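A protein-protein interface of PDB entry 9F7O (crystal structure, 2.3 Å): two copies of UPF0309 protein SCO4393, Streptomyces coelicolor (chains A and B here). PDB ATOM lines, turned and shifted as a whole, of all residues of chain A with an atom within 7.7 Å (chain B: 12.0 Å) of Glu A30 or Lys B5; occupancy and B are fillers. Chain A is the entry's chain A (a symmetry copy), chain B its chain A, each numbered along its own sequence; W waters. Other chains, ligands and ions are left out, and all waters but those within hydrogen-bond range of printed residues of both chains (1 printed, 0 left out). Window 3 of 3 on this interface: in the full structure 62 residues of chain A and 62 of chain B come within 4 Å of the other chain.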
ATOM      1  N   GLU A  25     -17.223 -14.824  33.790  1.00  0.00           N
ATOM      2  CA  GLU A  25     -15.994 -15.429  34.299  1.00  0.00           C
ATOM      3  C   GLU A  25     -14.718 -14.859  33.682  1.00  0.00           C
ATOM      4  O   GLU A  25     -13.639 -15.440  33.872  1.00  0.00           O
ATOM      5  CB  GLU A  25     -16.020 -16.941  34.062  1.00  0.00           C
ATOM      6  CG  GLU A  25     -17.187 -17.658  34.685  1.00  0.00           C
ATOM      7  CD  GLU A  25     -17.229 -17.464  36.200  1.00  0.00           C
ATOM      8  OE1 GLU A  25     -16.268 -17.886  36.888  1.00  0.00           O
ATOM      9  OE2 GLU A  25     -18.222 -16.895  36.706  1.00  0.00           O
ATOM     10  N   ALA A  26     -14.796 -13.744  32.957  1.00  0.00           N
ATOM     11  CA  ALA A  26     -13.611 -13.228  32.276  1.00  0.00           C
ATOM     12  C   ALA A  26     -12.486 -12.922  33.266  1.00  0.00           C
ATOM     13  O   ALA A  26     -11.305 -13.187  32.988  1.00  0.00           O
ATOM     14  CB  ALA A  26     -13.987 -11.984  31.466  1.00  0.00           C
ATOM     15  N   ASP A  27     -12.836 -12.395  34.439  1.00  0.00           N
ATOM     16  CA  ASP A  27     -11.815 -12.046  35.427  1.00  0.00           C
ATOM     17  C   ASP A  27     -11.231 -13.285  36.105  1.00  0.00           C
ATOM     18  O   ASP A  27     -10.025 -13.339  36.383  1.00  0.00           O
ATOM     19  CB  ASP A  27     -12.398 -11.108  36.486  1.00  0.00           C
ATOM     20  CG  ASP A  27     -12.662  -9.711  35.954  1.00  0.00           C
ATOM     21  OD1 ASP A  27     -12.045  -9.330  34.943  1.00  0.00           O
ATOM     22  OD2 ASP A  27     -13.481  -8.991  36.558  1.00  0.00           O
ATOM     23  N   SER A  28     -12.077 -14.267  36.424  1.00  0.00           N
ATOM     24  CA  SER A  28     -11.576 -15.491  37.040  1.00  0.00           C
ATOM     25  C   SER A  28     -10.776 -16.320  36.051  1.00  0.00           C
ATOM     26  O   SER A  28      -9.784 -16.952  36.434  1.00  0.00           O
ATOM     27  CB  SER A  28     -12.742 -16.299  37.605  1.00  0.00           C
ATOM     28  OG  SER A  28     -13.690 -16.608  36.586  1.00  0.00           O
ATOM     29  N   ILE A  29     -11.169 -16.312  34.772  1.00  0.00           N
ATOM     30  CA  ILE A  29     -10.384 -17.020  33.762  1.00  0.00           C
ATOM     31  C   ILE A  29      -8.998 -16.401  33.654  1.00  0.00           C
ATOM     32  O   ILE A  29      -7.990 -17.106  33.600  1.00  0.00           O
ATOM     33  CB  ILE A  29     -11.100 -17.017  32.400  1.00  0.00           C
ATOM     34  CG1 ILE A  29     -12.322 -17.921  32.408  1.00  0.00           C
ATOM     35  CG2 ILE A  29     -10.127 -17.402  31.292  1.00  0.00           C
ATOM     36  CD1 ILE A  29     -13.178 -17.745  31.188  1.00  0.00           C
ATOM     37  N   GLU A  30      -8.926 -15.075  33.598  1.00  0.00           N
ATOM     38  CA  GLU A  30      -7.622 -14.420  33.578  1.00  0.00           C
ATOM     39  C   GLU A  30      -6.818 -14.747  34.832  1.00  0.00           C
ATOM     40  O   GLU A  30      -5.617 -15.029  34.747  1.00  0.00           O
ATOM     41  CB  GLU A  30      -7.811 -12.910  33.430  1.00  0.00           C
ATOM     42  CG  GLU A  30      -6.523 -12.118  33.448  1.00  0.00           C
ATOM     43  CD  GLU A  30      -6.771 -10.653  33.148  1.00  0.00           C
ATOM     44  OE1 GLU A  30      -7.944 -10.291  32.913  1.00  0.00           O
ATOM     45  OE2 GLU A  30      -5.802  -9.861  33.140  1.00  0.00           O
ATOM     46  N   ALA A  31      -7.456 -14.708  36.007  1.00  0.00           N
ATOM     47  CA  ALA A  31      -6.746 -15.061  37.237  1.00  0.00           C
ATOM     48  C   ALA A  31      -6.178 -16.479  37.165  1.00  0.00           C
ATOM     49  O   ALA A  31      -5.023 -16.721  37.553  1.00  0.00           O
ATOM     50  CB  ALA A  31      -7.680 -14.909  38.440  1.00  0.00           C
ATOM     51  N   ALA A  32      -6.969 -17.429  36.663  1.00  0.00           N
ATOM     52  CA  ALA A  32      -6.479 -18.802  36.560  1.00  0.00           C
ATOM     53  C   ALA A  32      -5.353 -18.904  35.550  1.00  0.00           C
ATOM     54  O   ALA A  32      -4.303 -19.506  35.832  1.00  0.00           O
ATOM     55  CB  ALA A  32      -7.605 -19.752  36.174  1.00  0.00           C
ATOM     56  N   GLY A  33      -5.545 -18.318  34.364  1.00  0.00           N
ATOM     57  CA  GLY A  33      -4.466 -18.285  33.397  1.00  0.00           C
ATOM     58  C   GLY A  33      -3.211 -17.660  33.971  1.00  0.00           C
ATOM     59  O   GLY A  33      -2.097 -18.127  33.713  1.00  0.00           O
ATOM     60  N   THR A  34      -3.370 -16.590  34.753  1.00  0.00           N
ATOM     61  CA  THR A  34      -2.203 -15.960  35.363  1.00  0.00           C
ATOM     62  C   THR A  34      -1.529 -16.913  36.332  1.00  0.00           C
ATOM     63  O   THR A  34      -0.292 -16.980  36.394  1.00  0.00           O
ATOM     64  CB  THR A  34      -2.611 -14.674  36.076  1.00  0.00           C
ATOM     65  OG1 THR A  34      -3.139 -13.765  35.109  1.00  0.00           O
ATOM     66  CG2 THR A  34      -1.448 -14.033  36.816  1.00  0.00           C
ATOM     67  N   LEU A  35      -2.320 -17.655  37.106  1.00  0.00           N
ATOM     68  CA  LEU A  35      -1.721 -18.587  38.052  1.00  0.00           C
ATOM     69  C   LEU A  35      -0.916 -19.645  37.319  1.00  0.00           C
ATOM     70  O   LEU A  35       0.210 -19.964  37.705  1.00  0.00           O
ATOM     71  CB  LEU A  35      -2.792 -19.236  38.912  1.00  0.00           C
ATOM     72  CG  LEU A  35      -2.337 -20.391  39.782  1.00  0.00           C
ATOM     73  CD1 LEU A  35      -1.191 -20.020  40.648  1.00  0.00           C
ATOM     74  CD2 LEU A  35      -3.539 -20.795  40.633  1.00  0.00           C
ATOM     75  N   LEU A  36      -1.473 -20.193  36.243  1.00  0.00           N
ATOM     76  CA  LEU A  36      -0.715 -21.152  35.450  1.00  0.00           C
ATOM     77  C   LEU A  36       0.562 -20.519  34.907  1.00  0.00           C
ATOM     78  O   LEU A  36       1.640 -21.128  34.952  1.00  0.00           O
ATOM     79  CB  LEU A  36      -1.577 -21.701  34.309  1.00  0.00           C
ATOM     80  CG  LEU A  36      -2.870 -22.438  34.696  1.00  0.00           C
ATOM     81  CD1 LEU A  36      -3.582 -22.977  33.419  1.00  0.00           C
ATOM     82  CD2 LEU A  36      -2.643 -23.563  35.670  1.00  0.00           C
ATOM     83  N   ALA A  37       0.465 -19.291  34.388  1.00  0.00           N
ATOM     84  CA  ALA A  37       1.663 -18.610  33.895  1.00  0.00           C
ATOM     85  C   ALA A  37       2.689 -18.423  35.016  1.00  0.00           C
ATOM     86  O   ALA A  37       3.883 -18.703  34.846  1.00  0.00           O
ATOM     87  CB  ALA A  37       1.287 -17.264  33.274  1.00  0.00           C
ATOM     88  N   ILE A 169      -8.722 -20.632  43.224  1.00  0.00           N
ATOM     89  CA  ILE A 169      -9.503 -19.954  42.199  1.00  0.00           C
ATOM     90  C   ILE A 169     -10.648 -20.876  41.814  1.00  0.00           C
ATOM     91  O   ILE A 169     -10.454 -22.084  41.646  1.00  0.00           O
ATOM     92  CB  ILE A 169      -8.643 -19.586  40.982  1.00  0.00           C
ATOM     93  CG1 ILE A 169      -7.587 -18.590  41.421  1.00  0.00           C
ATOM     94  CG2 ILE A 169      -9.504 -18.982  39.925  1.00  0.00           C
ATOM     95  CD1 ILE A 169      -6.513 -18.328  40.395  1.00  0.00           C
ATOM     96  N   LEU A 171     -13.741 -21.392  39.028  1.00  0.00           N
ATOM     97  CA  LEU A 171     -14.342 -21.053  37.740  1.00  0.00           C
ATOM     98  C   LEU A 171     -15.722 -21.681  37.675  1.00  0.00           C
ATOM     99  O   LEU A 171     -15.832 -22.911  37.676  1.00  0.00           O
ATOM    100  CB  LEU A 171     -13.509 -21.556  36.564  1.00  0.00           C
ATOM    101  CG  LEU A 171     -12.050 -21.140  36.644  1.00  0.00           C
ATOM    102  CD1 LEU A 171     -11.202 -21.633  35.488  1.00  0.00           C
ATOM    103  CD2 LEU A 171     -11.953 -19.587  36.737  1.00  0.00           C
ATOM    104  N   ALA A 205     -10.035 -21.665  27.232  1.00  0.00           N
ATOM    105  CA  ALA A 205      -9.849 -20.246  27.529  1.00  0.00           C
ATOM    106  C   ALA A 205      -8.763 -20.045  28.573  1.00  0.00           C
ATOM    107  O   ALA A 205      -7.887 -19.184  28.430  1.00  0.00           O
ATOM    108  CB  ALA A 205     -11.170 -19.657  28.018  1.00  0.00           C
ATOM    109  N   VAL A 206      -8.798 -20.841  29.634  1.00  0.00           N
ATOM    110  CA  VAL A 206      -7.800 -20.708  30.685  1.00  0.00           C
ATOM    111  C   VAL A 206      -6.395 -20.940  30.135  1.00  0.00           C
ATOM    112  O   VAL A 206      -5.470 -20.168  30.406  1.00  0.00           O
ATOM    113  CB  VAL A 206      -8.099 -21.683  31.835  1.00  0.00           C
ATOM    114  CG1 VAL A 206      -6.877 -21.810  32.726  1.00  0.00           C
ATOM    115  CG2 VAL A 206      -9.326 -21.272  32.608  1.00  0.00           C
ATOM    116  N   THR A 209      -5.222 -18.240  27.857  1.00  0.00           N
ATOM    117  CA  THR A 209      -4.865 -17.055  28.627  1.00  0.00           C
ATOM    118  C   THR A 209      -3.475 -17.212  29.231  1.00  0.00           C
ATOM    119  O   THR A 209      -2.650 -16.292  29.171  1.00  0.00           O
ATOM    120  CB  THR A 209      -5.886 -16.792  29.738  1.00  0.00           C
ATOM    121  OG1 THR A 209      -7.187 -16.505  29.209  1.00  0.00           O
ATOM    122  CG2 THR A 209      -5.436 -15.596  30.597  1.00  0.00           C
ATOM    123  N   ALA A 210      -3.192 -18.378  29.824  1.00  0.00           N
ATOM    124  CA  ALA A 210      -1.856 -18.609  30.370  1.00  0.00           C
ATOM    125  C   ALA A 210      -0.791 -18.469  29.291  1.00  0.00           C
ATOM    126  O   ALA A 210       0.318 -17.981  29.557  1.00  0.00           O
ATOM    127  CB  ALA A 210      -1.750 -19.995  31.015  1.00  0.00           C
ATOM    128  N   ALA A 212      -0.897 -16.647  26.427  1.00  0.00           N
ATOM    129  CA  ALA A 212      -0.747 -15.245  26.061  1.00  0.00           C
ATOM    130  C   ALA A 212      -0.026 -14.470  27.160  1.00  0.00           C
ATOM    131  O   ALA A 212       0.822 -13.615  26.877  1.00  0.00           O
ATOM    132  CB  ALA A 212      -2.130 -14.660  25.774  1.00  0.00           C
ATOM    133  N   THR A 213      -0.338 -14.768  28.422  1.00  0.00           N
ATOM    134  CA  THR A 213       0.311 -14.067  29.525  1.00  0.00           C
ATOM    135  C   THR A 213       1.818 -14.289  29.516  1.00  0.00           C
ATOM    136  O   THR A 213       2.592 -13.341  29.685  1.00  0.00           O
ATOM    137  CB  THR A 213      -0.285 -14.512  30.854  1.00  0.00           C
ATOM    138  OG1 THR A 213      -1.626 -14.016  30.944  1.00  0.00           O
ATOM    139  CG2 THR A 213       0.547 -13.981  32.016  1.00  0.00           C
ATOM    140  N   HIS B   4      -9.564  -7.373  22.404  1.00  0.00           N
ATOM    141  CA  HIS B   4     -10.152  -8.042  23.558  1.00  0.00           C
ATOM    142  C   HIS B   4      -9.180  -9.077  24.135  1.00  0.00           C
ATOM    143  O   HIS B   4      -8.095  -9.310  23.596  1.00  0.00           O
ATOM    144  CB  HIS B   4     -11.474  -8.722  23.175  1.00  0.00           C
ATOM    145  CG  HIS B   4     -12.546  -7.771  22.732  1.00  0.00           C
ATOM    146  ND1 HIS B   4     -12.287  -6.669  21.944  1.00  0.00           N
ATOM    147  CD2 HIS B   4     -13.882  -7.767  22.955  1.00  0.00           C
ATOM    148  CE1 HIS B   4     -13.414  -6.022  21.710  1.00  0.00           C
ATOM    149  NE2 HIS B   4     -14.398  -6.668  22.311  1.00  0.00           N
ATOM    150  N   LYS B   5      -9.591  -9.715  25.219  1.00  0.00           N
ATOM    151  CA  LYS B   5      -8.743 -10.667  25.912  1.00  0.00           C
ATOM    152  C   LYS B   5      -8.863 -12.059  25.297  1.00  0.00           C
ATOM    153  O   LYS B   5      -9.884 -12.392  24.691  1.00  0.00           O
ATOM    154  CB  LYS B   5      -9.123 -10.728  27.382  1.00  0.00           C
ATOM    155  CG  LYS B   5      -8.932  -9.410  28.106  1.00  0.00           C
ATOM    156  CD  LYS B   5      -9.621  -9.428  29.464  1.00  0.00           C
ATOM    157  CE  LYS B   5      -9.416  -8.118  30.216  1.00  0.00           C
ATOM    158  NZ  LYS B   5      -7.955  -7.808  30.389  1.00  0.00           N
ATOM    159  N   PRO B   6      -7.833 -12.895  25.461  1.00  0.00           N
ATOM    160  CA  PRO B   6      -7.833 -14.187  24.737  1.00  0.00           C
ATOM    161  C   PRO B   6      -8.998 -15.086  25.113  1.00  0.00           C
ATOM    162  O   PRO B   6      -9.543 -15.785  24.251  1.00  0.00           O
ATOM    163  CB  PRO B   6      -6.483 -14.822  25.110  1.00  0.00           C
ATOM    164  CG  PRO B   6      -5.659 -13.701  25.681  1.00  0.00           C
ATOM    165  CD  PRO B   6      -6.604 -12.668  26.242  1.00  0.00           C
ATOM    166  N   ALA B   7      -9.407 -15.086  26.379  1.00  0.00           N
ATOM    167  CA  ALA B   7     -10.530 -15.928  26.767  1.00  0.00           C
ATOM    168  C   ALA B   7     -11.790 -15.571  25.980  1.00  0.00           C
ATOM    169  O   ALA B   7     -12.493 -16.450  25.472  1.00  0.00           O
ATOM    170  CB  ALA B   7     -10.784 -15.809  28.265  1.00  0.00           C
ATOM    171  N   GLY B   8     -12.116 -14.288  25.898  1.00  0.00           N
ATOM    172  CA  GLY B   8     -13.351 -13.910  25.231  1.00  0.00           C
ATOM    173  C   GLY B   8     -13.315 -14.072  23.723  1.00  0.00           C
ATOM    174  O   GLY B   8     -14.342 -14.361  23.104  1.00  0.00           O
ATOM    175  N   GLN B   9     -12.147 -13.873  23.112  1.00  0.00           N
ATOM    176  CA  GLN B   9     -12.003 -14.159  21.693  1.00  0.00           C
ATOM    177  C   GLN B   9     -12.204 -15.639  21.431  1.00  0.00           C
ATOM    178  O   GLN B   9     -12.949 -16.022  20.520  1.00  0.00           O
ATOM    179  CB  GLN B   9     -10.632 -13.713  21.199  1.00  0.00           C
ATOM    180  CG  GLN B   9     -10.390 -12.234  21.306  1.00  0.00           C
ATOM    181  CD  GLN B   9      -9.083 -11.817  20.652  1.00  0.00           C
ATOM    182  OE1 GLN B   9      -9.035 -11.528  19.458  1.00  0.00           O
ATOM    183  NE2 GLN B   9      -8.016 -11.803  21.429  1.00  0.00           N
ATOM    184  N   PHE B  10     -11.567 -16.493  22.233  1.00  0.00           N
ATOM    185  CA  PHE B  10     -11.747 -17.927  22.043  1.00  0.00           C
ATOM    186  C   PHE B  10     -13.205 -18.328  22.230  1.00  0.00           C
ATOM    187  O   PHE B  10     -13.760 -19.095  21.431  1.00  0.00           O
ATOM    188  CB  PHE B  10     -10.873 -18.746  23.001  1.00  0.00           C
ATOM    189  CG  PHE B  10     -11.182 -20.217  22.926  1.00  0.00           C
ATOM    190  CD1 PHE B  10     -10.604 -21.003  21.948  1.00  0.00           C
ATOM    191  CD2 PHE B  10     -12.114 -20.788  23.777  1.00  0.00           C
ATOM    192  CE1 PHE B  10     -10.910 -22.324  21.833  1.00  0.00           C
ATOM    193  CE2 PHE B  10     -12.438 -22.122  23.668  1.00  0.00           C
ATOM    194  CZ  PHE B  10     -11.835 -22.893  22.674  1.00  0.00           C
ATOM    195  N   LEU B  11     -13.841 -17.837  23.296  1.00  0.00           N
ATOM    196  CA  LEU B  11     -15.233 -18.200  23.542  1.00  0.00           C
ATOM    197  C   LEU B  11     -16.146 -17.699  22.426  1.00  0.00           C
ATOM    198  O   LEU B  11     -17.127 -18.374  22.077  1.00  0.00           O
ATOM    199  CB  LEU B  11     -15.703 -17.658  24.892  1.00  0.00           C
ATOM    200  CG  LEU B  11     -15.026 -18.244  26.130  1.00  0.00           C
ATOM    201  CD1 LEU B  11     -15.308 -17.441  27.391  1.00  0.00           C
ATOM    202  CD2 LEU B  11     -15.453 -19.708  26.356  1.00  0.00           C
ATOM    203  N   ASP B  12     -15.852 -16.507  21.863  1.00  0.00           N
ATOM    204  CA  ASP B  12     -16.635 -16.013  20.729  1.00  0.00           C
ATOM    205  C   ASP B  12     -16.430 -16.902  19.506  1.00  0.00           C
ATOM    206  O   ASP B  12     -17.374 -17.162  18.750  1.00  0.00           O
ATOM    207  CB  ASP B  12     -16.257 -14.570  20.389  1.00  0.00           C
ATOM    208  CG  ASP B  12     -16.913 -13.533  21.301  1.00  0.00           C
ATOM    209  OD1 ASP B  12     -18.023 -13.764  21.838  1.00  0.00           O
ATOM    210  OD2 ASP B  12     -16.315 -12.451  21.428  1.00  0.00           O
ATOM    211  N   ALA B  13     -15.200 -17.370  19.286  1.00  0.00           N
ATOM    212  CA  ALA B  13     -14.961 -18.277  18.166  1.00  0.00           C
ATOM    213  C   ALA B  13     -15.720 -19.588  18.341  1.00  0.00           C
ATOM    214  O   ALA B  13     -16.237 -20.149  17.371  1.00  0.00           O
ATOM    215  CB  ALA B  13     -13.469 -18.562  18.012  1.00  0.00           C
ATOM    216  N   ALA B  14     -15.801 -20.098  19.573  1.00  0.00           N
ATOM    217  CA  ALA B  14     -16.583 -21.310  19.795  1.00  0.00           C
ATOM    218  C   ALA B  14     -18.066 -21.045  19.597  1.00  0.00           C
ATOM    219  O   ALA B  14     -18.789 -21.890  19.056  1.00  0.00           O
ATOM    220  CB  ALA B  14     -16.354 -21.868  21.199  1.00  0.00           C
ATOM    221  N   ILE B  15     -18.545 -19.890  20.054  1.00  0.00           N
ATOM    222  CA  ILE B  15     -19.961 -19.576  19.884  1.00  0.00           C
ATOM    223  C   ILE B  15     -20.309 -19.515  18.406  1.00  0.00           C
ATOM    224  O   ILE B  15     -21.367 -20.001  17.989  1.00  0.00           O
ATOM    225  CB  ILE B  15     -20.339 -18.261  20.589  1.00  0.00           C
ATOM    226  CG1 ILE B  15     -20.293 -18.449  22.094  1.00  0.00           C
ATOM    227  CG2 ILE B  15     -21.705 -17.778  20.083  1.00  0.00           C
ATOM    228  CD1 ILE B  15     -20.070 -17.149  22.851  1.00  0.00           C
ATOM    229  N   GLU B 181      -8.007 -21.338  16.942  1.00  0.00           N
ATOM    230  CA  GLU B 181      -8.931 -20.213  16.808  1.00  0.00           C
ATOM    231  C   GLU B 181      -8.319 -18.868  17.164  1.00  0.00           C
ATOM    232  O   GLU B 181      -8.950 -17.832  16.924  1.00  0.00           O
ATOM    233  CB  GLU B 181     -10.173 -20.445  17.681  1.00  0.00           C
ATOM    234  CG  GLU B 181     -10.964 -21.691  17.302  1.00  0.00           C
ATOM    235  CD  GLU B 181     -11.324 -21.707  15.853  1.00  0.00           C
ATOM    236  OE1 GLU B 181     -11.655 -20.631  15.315  1.00  0.00           O
ATOM    237  OE2 GLU B 181     -11.255 -22.795  15.260  1.00  0.00           O
ATOM    238  N   LEU B 182      -7.129 -18.853  17.734  1.00  0.00           N
ATOM    239  CA  LEU B 182      -6.525 -17.627  18.208  1.00  0.00           C
ATOM    240  C   LEU B 182      -5.165 -17.419  17.563  1.00  0.00           C
ATOM    241  O   LEU B 182      -4.422 -18.365  17.298  1.00  0.00           O
ATOM    242  CB  LEU B 182      -6.368 -17.637  19.729  1.00  0.00           C
ATOM    243  CG  LEU B 182      -7.656 -17.665  20.556  1.00  0.00           C
ATOM    244  CD1 LEU B 182      -7.280 -17.736  22.050  1.00  0.00           C
ATOM    245  CD2 LEU B 182      -8.526 -16.464  20.265  1.00  0.00           C
ATOM    246  N   THR B 183      -4.844 -16.157  17.319  1.00  0.00           N
ATOM    247  CA  THR B 183      -3.544 -15.760  16.806  1.00  0.00           C
ATOM    248  C   THR B 183      -3.087 -14.555  17.605  1.00  0.00           C
ATOM    249  O   THR B 183      -3.871 -13.633  17.852  1.00  0.00           O
ATOM    250  CB  THR B 183      -3.607 -15.454  15.309  1.00  0.00           C
ATOM    251  OG1 THR B 183      -4.895 -14.919  14.982  1.00  0.00           O
ATOM    252  CG2 THR B 183      -3.389 -16.750  14.537  1.00  0.00           C
ATOM    253  N   LEU B 184      -1.842 -14.585  18.047  1.00  0.00           N
ATOM    254  CA  LEU B 184      -1.270 -13.494  18.818  1.00  0.00           C
ATOM    255  C   LEU B 184      -0.089 -12.935  18.052  1.00  0.00           C
ATOM    256  O   LEU B 184       0.729 -13.700  17.533  1.00  0.00           O
ATOM    257  CB  LEU B 184      -0.827 -13.964  20.195  1.00  0.00           C
ATOM    258  CG  LEU B 184      -1.732 -13.568  21.361  1.00  0.00           C
ATOM    259  CD1 LEU B 184      -3.146 -13.986  21.126  1.00  0.00           C
ATOM    260  CD2 LEU B 184      -1.133 -14.204  22.642  1.00  0.00           C
ATOM    261  N   ASP B 185      -0.023 -11.604  17.964  1.00  0.00           N
ATOM    262  CA  ASP B 185       1.128 -10.959  17.341  1.00  0.00           C
ATOM    263  C   ASP B 185       2.425 -11.490  17.927  1.00  0.00           C
ATOM    264  O   ASP B 185       3.405 -11.702  17.206  1.00  0.00           O
ATOM    265  CB  ASP B 185       1.013  -9.446  17.518  1.00  0.00           C
ATOM    266  CG  ASP B 185      -0.283  -8.895  16.938  1.00  0.00           C
ATOM    267  OD1 ASP B 185      -1.373  -9.320  17.394  1.00  0.00           O
ATOM    268  OD2 ASP B 185      -0.209  -8.045  16.024  1.00  0.00           O
ATOM    269  N   THR B 186       2.430 -11.752  19.233  1.00  0.00           N
ATOM    270  CA  THR B 186       3.609 -12.321  19.874  1.00  0.00           C
ATOM    271  C   THR B 186       3.866 -13.752  19.399  1.00  0.00           C
ATOM    272  O   THR B 186       4.999 -14.117  19.064  1.00  0.00           O
ATOM    273  CB  THR B 186       3.436 -12.267  21.397  1.00  0.00           C
ATOM    274  OG1 THR B 186       2.262 -13.001  21.784  1.00  0.00           O
ATOM    275  CG2 THR B 186       3.285 -10.826  21.887  1.00  0.00           C
ATOM    276  N   PHE B 191      -3.102 -20.940  17.970  1.00  0.00           N
ATOM    277  CA  PHE B 191      -3.321 -21.854  19.082  1.00  0.00           C
ATOM    278  C   PHE B 191      -4.792 -21.796  19.485  1.00  0.00           C
ATOM    279  O   PHE B 191      -5.596 -21.070  18.881  1.00  0.00           O
ATOM    280  CB  PHE B 191      -2.367 -21.542  20.258  1.00  0.00           C
ATOM    281  CG  PHE B 191      -2.550 -20.169  20.859  1.00  0.00           C
ATOM    282  CD1 PHE B 191      -2.096 -19.050  20.189  1.00  0.00           C
ATOM    283  CD2 PHE B 191      -3.181 -19.999  22.085  1.00  0.00           C
ATOM    284  CE1 PHE B 191      -2.272 -17.785  20.714  1.00  0.00           C
ATOM    285  CE2 PHE B 191      -3.362 -18.731  22.620  1.00  0.00           C
ATOM    286  CZ  PHE B 191      -2.908 -17.624  21.926  1.00  0.00           C
ATOM    287  N   ALA B 192      -5.152 -22.638  20.478  1.00  0.00           N
ATOM    288  CA  ALA B 192      -6.465 -22.652  21.123  1.00  0.00           C
ATOM    289  C   ALA B 192      -7.518 -23.406  20.314  1.00  0.00           C
ATOM    290  O   ALA B 192      -8.343 -22.811  19.601  1.00  0.00           O
ATOM    291  CB  ALA B 192      -6.944 -21.226  21.398  1.00  0.00           C
HETATM  292  O   HOH W   1      -8.221 -13.920  28.968  1.00  0.00           O
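NZ of Lys B5 is in salt-bridge range of OE1 of Glu A30, 3.5 Å away.
Among the printed residues, 6 pairs touch across the chains. Among the printed residues, Asp or Glu carboxylates within 4 Å of a Lys or Arg side-chain nitrogen of the other chain: Glu A30 with Lys B5 (3.5 Å).
Water W1 bridges the side-chain hydroxyl of Thr A209 (2.8 Å) and the backbone NH of Ala B7 (3.1 Å).
No position is printed for both chains. Of the 6 pairs that touch across the chains among the printed residues, none has its exchanged pair printed and touching as well.
Of the printed residues of chain B, Glu A30 touches Lys B5. Of chain A, only Glu A30 (3.5 Å) comes within 4 Å of Lys B5. No residue of chain B comes within 4 Å of Ala A26. No residue of chain B comes within 4 Å of Asp A27. No residue of chain B comes within 4 Å of Ala A32. Gly A33 touches none of the printed residues of chain B. Thr A34 touches none of the printed residues of chain B. No residue of chain B comes within 4 Å of Val A206. Of chain B, only Ala B7 (3.8 Å) comes within 4 Å of Thr A209. Printed residues of chain A within 4 Å of Pro B6: Ala A212 (3.7 Å). Of the printed residues of chain A, Ala B7 touches Ile A29 (3.5 Å), Ala A205 (3.9 Å) and Thr A209 (3.8 Å). Of the printed residues of chain B, Ala A205 touches Ala B7 (3.9 Å). The nearest residue of chain A that does not touch Lys B5 is Ala A26 (5.4 Å).
Among the printed residues, merely in contact across the chains: Ala A212 with Leu B184, Ile A29 with Ala B7, Ala A212 with Pro B6, Thr A209 with Ala B7 and Ala A205 with Ala B7.
The side-chain hydroxyl (OG1) of Thr A34 sits at hydrogen-bond distance from the backbone carbonyl oxygen (O) of Glu A30 (2.8 Å). O of Ala A205 sits at hydrogen-bond distance from OG1 of Thr A209 (2.9 Å). O of Thr A209 sits at hydrogen-bond distance from OG1 of Thr A213, at 3.1 Å.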
